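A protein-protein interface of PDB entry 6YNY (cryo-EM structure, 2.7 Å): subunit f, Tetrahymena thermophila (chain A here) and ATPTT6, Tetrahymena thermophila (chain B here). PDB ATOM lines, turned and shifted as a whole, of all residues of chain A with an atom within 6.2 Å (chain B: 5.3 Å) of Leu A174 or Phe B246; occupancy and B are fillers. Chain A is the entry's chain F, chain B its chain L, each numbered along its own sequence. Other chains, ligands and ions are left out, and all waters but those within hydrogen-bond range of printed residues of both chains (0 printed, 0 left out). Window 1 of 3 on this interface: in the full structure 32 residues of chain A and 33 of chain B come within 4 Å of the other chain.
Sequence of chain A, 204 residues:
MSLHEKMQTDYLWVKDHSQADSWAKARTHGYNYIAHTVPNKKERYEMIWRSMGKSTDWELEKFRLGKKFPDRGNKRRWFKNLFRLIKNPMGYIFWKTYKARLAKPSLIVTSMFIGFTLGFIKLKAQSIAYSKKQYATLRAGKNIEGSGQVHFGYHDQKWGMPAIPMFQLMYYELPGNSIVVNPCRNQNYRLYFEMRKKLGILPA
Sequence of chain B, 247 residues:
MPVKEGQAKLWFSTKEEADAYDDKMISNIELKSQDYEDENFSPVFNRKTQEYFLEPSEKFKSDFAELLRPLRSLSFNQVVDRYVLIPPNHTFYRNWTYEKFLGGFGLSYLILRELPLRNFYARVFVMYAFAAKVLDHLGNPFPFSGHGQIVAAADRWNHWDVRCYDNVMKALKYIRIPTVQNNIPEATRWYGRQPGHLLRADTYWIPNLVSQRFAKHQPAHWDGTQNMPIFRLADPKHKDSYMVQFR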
ATOM      1  N   LYS A 158     -17.403  16.672  36.598  1.00  0.00           N
ATOM      2  CA  LYS A 158     -16.526  16.219  35.526  1.00  0.00           C
ATOM      3  C   LYS A 158     -15.303  17.123  35.532  1.00  0.00           C
ATOM      4  O   LYS A 158     -15.400  18.309  35.208  1.00  0.00           O
ATOM      5  CB  LYS A 158     -17.226  16.234  34.173  1.00  0.00           C
ATOM      6  CG  LYS A 158     -16.783  15.087  33.288  1.00  0.00           C
ATOM      7  CD  LYS A 158     -17.560  15.023  32.000  1.00  0.00           C
ATOM      8  CE  LYS A 158     -17.249  16.209  31.138  1.00  0.00           C
ATOM      9  NZ  LYS A 158     -17.753  16.019  29.766  1.00  0.00           N
ATOM     10  N   TYR A 172     -12.147  12.202  23.543  1.00  0.00           N
ATOM     11  CA  TYR A 172     -11.765  13.403  22.821  1.00  0.00           C
ATOM     12  C   TYR A 172     -12.889  14.419  22.936  1.00  0.00           C
ATOM     13  O   TYR A 172     -14.069  14.065  22.983  1.00  0.00           O
ATOM     14  CB  TYR A 172     -11.430  13.122  21.352  1.00  0.00           C
ATOM     15  CG  TYR A 172     -12.585  12.737  20.461  1.00  0.00           C
ATOM     16  CD1 TYR A 172     -13.362  13.703  19.849  1.00  0.00           C
ATOM     17  CD2 TYR A 172     -12.872  11.410  20.199  1.00  0.00           C
ATOM     18  CE1 TYR A 172     -14.400  13.358  19.023  1.00  0.00           C
ATOM     19  CE2 TYR A 172     -13.907  11.060  19.374  1.00  0.00           C
ATOM     20  CZ  TYR A 172     -14.668  12.036  18.787  1.00  0.00           C
ATOM     21  OH  TYR A 172     -15.703  11.682  17.963  1.00  0.00           O
ATOM     22  N   GLU A 173     -12.502  15.689  22.993  1.00  0.00           N
ATOM     23  CA  GLU A 173     -13.451  16.762  23.236  1.00  0.00           C
ATOM     24  C   GLU A 173     -14.418  16.915  22.070  1.00  0.00           C
ATOM     25  O   GLU A 173     -14.118  16.562  20.927  1.00  0.00           O
ATOM     26  CB  GLU A 173     -12.711  18.074  23.474  1.00  0.00           C
ATOM     27  CG  GLU A 173     -11.796  18.046  24.683  1.00  0.00           C
ATOM     28  CD  GLU A 173     -12.552  17.971  25.992  1.00  0.00           C
ATOM     29  OE1 GLU A 173     -13.708  18.439  26.042  1.00  0.00           O
ATOM     30  OE2 GLU A 173     -11.990  17.442  26.971  1.00  0.00           O
ATOM     31  N   LEU A 174     -15.585  17.456  22.375  1.00  0.00           N
ATOM     32  CA  LEU A 174     -16.641  17.654  21.396  1.00  0.00           C
ATOM     33  C   LEU A 174     -16.265  18.734  20.393  1.00  0.00           C
ATOM     34  O   LEU A 174     -16.165  19.905  20.777  1.00  0.00           O
ATOM     35  CB  LEU A 174     -17.930  18.023  22.115  1.00  0.00           C
ATOM     36  CG  LEU A 174     -19.112  18.475  21.265  1.00  0.00           C
ATOM     37  CD1 LEU A 174     -19.465  17.444  20.223  1.00  0.00           C
ATOM     38  CD2 LEU A 174     -20.291  18.737  22.165  1.00  0.00           C
ATOM     39  N   PRO A 175     -16.047  18.406  19.116  1.00  0.00           N
ATOM     40  CA  PRO A 175     -15.782  19.443  18.111  1.00  0.00           C
ATOM     41  C   PRO A 175     -17.079  20.040  17.593  1.00  0.00           C
ATOM     42  O   PRO A 175     -17.885  19.358  16.952  1.00  0.00           O
ATOM     43  CB  PRO A 175     -15.019  18.680  17.021  1.00  0.00           C
ATOM     44  CG  PRO A 175     -15.309  17.227  17.250  1.00  0.00           C
ATOM     45  CD  PRO A 175     -16.111  17.073  18.500  1.00  0.00           C
ATOM     46  N   GLY A 176     -17.287  21.326  17.876  1.00  0.00           N
ATOM     47  CA  GLY A 176     -18.531  21.969  17.496  1.00  0.00           C
ATOM     48  C   GLY A 176     -18.760  22.012  16.000  1.00  0.00           C
ATOM     49  O   GLY A 176     -19.904  22.054  15.546  1.00  0.00           O
ATOM     50  N   ASN A 177     -17.683  22.007  15.216  1.00  0.00           N
ATOM     51  CA  ASN A 177     -17.803  22.059  13.766  1.00  0.00           C
ATOM     52  C   ASN A 177     -18.350  20.769  13.176  1.00  0.00           C
ATOM     53  O   ASN A 177     -18.653  20.737  11.980  1.00  0.00           O
ATOM     54  CB  ASN A 177     -16.443  22.387  13.151  1.00  0.00           C
ATOM     55  CG  ASN A 177     -16.533  22.718  11.682  1.00  0.00           C
ATOM     56  OD1 ASN A 177     -17.065  23.759  11.302  1.00  0.00           O
ATOM     57  ND2 ASN A 177     -15.988  21.849  10.845  1.00  0.00           N
ATOM     58  N   SER A 178     -18.482  19.717  13.976  1.00  0.00           N
ATOM     59  CA  SER A 178     -19.048  18.457  13.523  1.00  0.00           C
ATOM     60  C   SER A 178     -20.554  18.376  13.722  1.00  0.00           C
ATOM     61  O   SER A 178     -21.175  17.429  13.231  1.00  0.00           O
ATOM     62  CB  SER A 178     -18.373  17.295  14.249  1.00  0.00           C
ATOM     63  OG  SER A 178     -16.994  17.240  13.939  1.00  0.00           O
ATOM     64  N   ILE A 179     -21.148  19.329  14.430  1.00  0.00           N
ATOM     65  CA  ILE A 179     -22.595  19.405  14.583  1.00  0.00           C
ATOM     66  C   ILE A 179     -23.140  20.206  13.410  1.00  0.00           C
ATOM     67  O   ILE A 179     -22.806  21.383  13.241  1.00  0.00           O
ATOM     68  CB  ILE A 179     -22.981  20.043  15.924  1.00  0.00           C
ATOM     69  CG1 ILE A 179     -22.473  19.186  17.079  1.00  0.00           C
ATOM     70  CG2 ILE A 179     -24.478  20.199  16.020  1.00  0.00           C
ATOM     71  CD1 ILE A 179     -22.500  19.871  18.417  1.00  0.00           C
ATOM     72  N   LEU B 198     -24.628  14.707  14.578  1.00  0.00           N
ATOM     73  CA  LEU B 198     -23.182  14.748  14.710  1.00  0.00           C
ATOM     74  C   LEU B 198     -22.564  13.852  13.650  1.00  0.00           C
ATOM     75  O   LEU B 198     -22.990  12.707  13.475  1.00  0.00           O
ATOM     76  CB  LEU B 198     -22.764  14.311  16.112  1.00  0.00           C
ATOM     77  CG  LEU B 198     -21.290  14.380  16.489  1.00  0.00           C
ATOM     78  CD1 LEU B 198     -20.800  15.799  16.485  1.00  0.00           C
ATOM     79  CD2 LEU B 198     -21.087  13.757  17.844  1.00  0.00           C
ATOM     80  N   ALA B 234     -25.725  13.927  18.703  1.00  0.00           N
ATOM     81  CA  ALA B 234     -24.935  14.673  19.680  1.00  0.00           C
ATOM     82  C   ALA B 234     -25.564  14.522  21.064  1.00  0.00           C
ATOM     83  O   ALA B 234     -26.115  15.456  21.649  1.00  0.00           O
ATOM     84  CB  ALA B 234     -24.827  16.134  19.274  1.00  0.00           C
ATOM     85  N   ASP B 235     -25.469  13.300  21.590  1.00  0.00           N
ATOM     86  CA  ASP B 235     -25.951  12.990  22.918  1.00  0.00           C
ATOM     87  C   ASP B 235     -24.886  12.151  23.617  1.00  0.00           C
ATOM     88  O   ASP B 235     -24.351  11.207  23.010  1.00  0.00           O
ATOM     89  CB  ASP B 235     -27.283  12.242  22.872  1.00  0.00           C
ATOM     90  CG  ASP B 235     -27.950  12.147  24.229  1.00  0.00           C
ATOM     91  OD1 ASP B 235     -28.737  13.054  24.570  1.00  0.00           O
ATOM     92  OD2 ASP B 235     -27.685  11.173  24.959  1.00  0.00           O
ATOM     93  N   PRO B 236     -24.551  12.462  24.871  1.00  0.00           N
ATOM     94  CA  PRO B 236     -23.499  11.697  25.558  1.00  0.00           C
ATOM     95  C   PRO B 236     -23.791  10.215  25.670  1.00  0.00           C
ATOM     96  O   PRO B 236     -22.854   9.416  25.785  1.00  0.00           O
ATOM     97  CB  PRO B 236     -23.435  12.356  26.940  1.00  0.00           C
ATOM     98  CG  PRO B 236     -24.053  13.670  26.779  1.00  0.00           C
ATOM     99  CD  PRO B 236     -25.073  13.547  25.713  1.00  0.00           C
ATOM    100  N   SER B 241     -21.230   8.013  20.284  1.00  0.00           N
ATOM    101  CA  SER B 241     -20.735   9.304  20.738  1.00  0.00           C
ATOM    102  C   SER B 241     -20.289   9.277  22.193  1.00  0.00           C
ATOM    103  O   SER B 241     -19.954  10.331  22.743  1.00  0.00           O
ATOM    104  CB  SER B 241     -21.807  10.379  20.553  1.00  0.00           C
ATOM    105  OG  SER B 241     -22.287  10.401  19.225  1.00  0.00           O
ATOM    106  N   VAL B 244     -17.069  10.982  23.209  1.00  0.00           N
ATOM    107  CA  VAL B 244     -17.013  12.434  23.134  1.00  0.00           C
ATOM    108  C   VAL B 244     -17.356  13.008  24.498  1.00  0.00           C
ATOM    109  O   VAL B 244     -18.287  12.550  25.168  1.00  0.00           O
ATOM    110  CB  VAL B 244     -17.967  12.954  22.046  1.00  0.00           C
ATOM    111  CG1 VAL B 244     -17.862  14.451  21.920  1.00  0.00           C
ATOM    112  CG2 VAL B 244     -17.665  12.284  20.730  1.00  0.00           C
ATOM    113  N   GLN B 245     -16.596  14.016  24.911  1.00  0.00           N
ATOM    114  CA  GLN B 245     -16.750  14.620  26.226  1.00  0.00           C
ATOM    115  C   GLN B 245     -17.656  15.839  26.121  1.00  0.00           C
ATOM    116  O   GLN B 245     -17.309  16.823  25.461  1.00  0.00           O
ATOM    117  CB  GLN B 245     -15.389  14.999  26.797  1.00  0.00           C
ATOM    118  CG  GLN B 245     -14.454  13.825  26.958  1.00  0.00           C
ATOM    119  CD  GLN B 245     -14.980  12.789  27.925  1.00  0.00           C
ATOM    120  OE1 GLN B 245     -15.686  11.859  27.535  1.00  0.00           O
ATOM    121  NE2 GLN B 245     -14.636  12.940  29.194  1.00  0.00           N
ATOM    122  N   PHE B 246     -18.811  15.767  26.771  1.00  0.00           N
ATOM    123  CA  PHE B 246     -19.791  16.845  26.769  1.00  0.00           C
ATOM    124  C   PHE B 246     -19.693  17.587  28.096  1.00  0.00           C
ATOM    125  O   PHE B 246     -20.143  17.084  29.130  1.00  0.00           O
ATOM    126  CB  PHE B 246     -21.197  16.291  26.547  1.00  0.00           C
ATOM    127  CG  PHE B 246     -21.380  15.612  25.226  1.00  0.00           C
ATOM    128  CD1 PHE B 246     -22.098  16.221  24.220  1.00  0.00           C
ATOM    129  CD2 PHE B 246     -20.838  14.367  24.988  1.00  0.00           C
ATOM    130  CE1 PHE B 246     -22.270  15.601  23.008  1.00  0.00           C
ATOM    131  CE2 PHE B 246     -21.009  13.749  23.774  1.00  0.00           C
ATOM    132  CZ  PHE B 246     -21.725  14.366  22.786  1.00  0.00           C
ATOM    133  N   ARG B 247     -19.103  18.776  28.064  1.00  0.00           N
ATOM    134  CA  ARG B 247     -18.899  19.565  29.273  1.00  0.00           C
ATOM    135  C   ARG B 247     -19.376  20.999  29.088  1.00  0.00           C
ATOM    136  O   ARG B 247     -20.400  21.399  29.643  1.00  0.00           O
ATOM    137  CB  ARG B 247     -17.424  19.543  29.680  1.00  0.00           C
ATOM    138  CG  ARG B 247     -16.453  19.736  28.540  1.00  0.00           C
ATOM    139  CD  ARG B 247     -15.011  19.577  28.994  1.00  0.00           C
ATOM    140  NE  ARG B 247     -14.741  18.244  29.516  1.00  0.00           N
ATOM    141  CZ  ARG B 247     -13.525  17.738  29.671  1.00  0.00           C
ATOM    142  NH1 ARG B 247     -12.456  18.448  29.344  1.00  0.00           N
ATOM    143  NH2 ARG B 247     -13.379  16.515  30.152  1.00  0.00           N
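Printed residues of chain B that touch a printed residue of chain A: Leu B198, Val B244, Gln B245, Phe B246 and Arg B247.
Hydrophobic or aromatic side chains of chain B that line the printed part of chain A: Leu B198, Val B244 and Phe B246.
Of the 9 printed residues of chain A, 6 touch a printed residue of chain B.
Printed residues of chain A that touch a printed residue of chain B: Lys A158, Tyr A172, Glu A173, Leu A174, Ser A178 and Ile A179.
Among the printed residues, 12 pairs touch across the chains.
Leu A174 touches just these residues of chain B: Val B244, Gln B245 and Phe B246.
Of the printed residues of chain B, Ser A178 touches Leu B198.
Printed residues of chain B within 4 Å of Ile A179: Leu B198 (3.8 Å).
Of the printed residues of chain A, Leu B198 touches Ser A178 (3.6 Å) and Ile A179 (3.8 Å).
Ala B234 touches none of the printed residues of chain A.
Printed residues of chain A within 4 Å of Gln B245: Lys A158, Tyr A172, Glu A173 and Leu A174.
Phe B246 touches just these residues of chain A: Lys A158 and Leu A174.
Of the printed residues of chain A, Arg B247 touches Lys A158 and Glu A173.
The nearest printed residue of chain B that does not touch Lys A158 is Val B244 (5.8 Å).
The backbone NH of Gln B245 lies within hydrogen-bond range of the backbone carbonyl oxygen of Tyr A172, at 3.2 Å.
NZ of Lys A158 sits at hydrogen-bond distance from O of Phe B246.
The guanidinium group (NH1) of Arg B247 is in salt-bridge range of the side-chain carboxylate (OE2) of Glu A173, 2.6 Å away.
C of Gln B245 touches NZ of Lys A158, at 3.7 Å.
N of Arg B247 touches NZ of Lys A158 (3.5 Å).
Val B244 touches Tyr A172 (CA to O, 3.4 Å).
OE1 of Glu A173 touches CB of Gln B245 (3.9 Å).
Leu A174 touches Val B244.
Gln B245 touches Leu A174 (O to N, 3.6 Å).
Phe B246 touches Leu A174.
Leu B198 touches Ser A178.
Ile A179 touches Leu B198.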
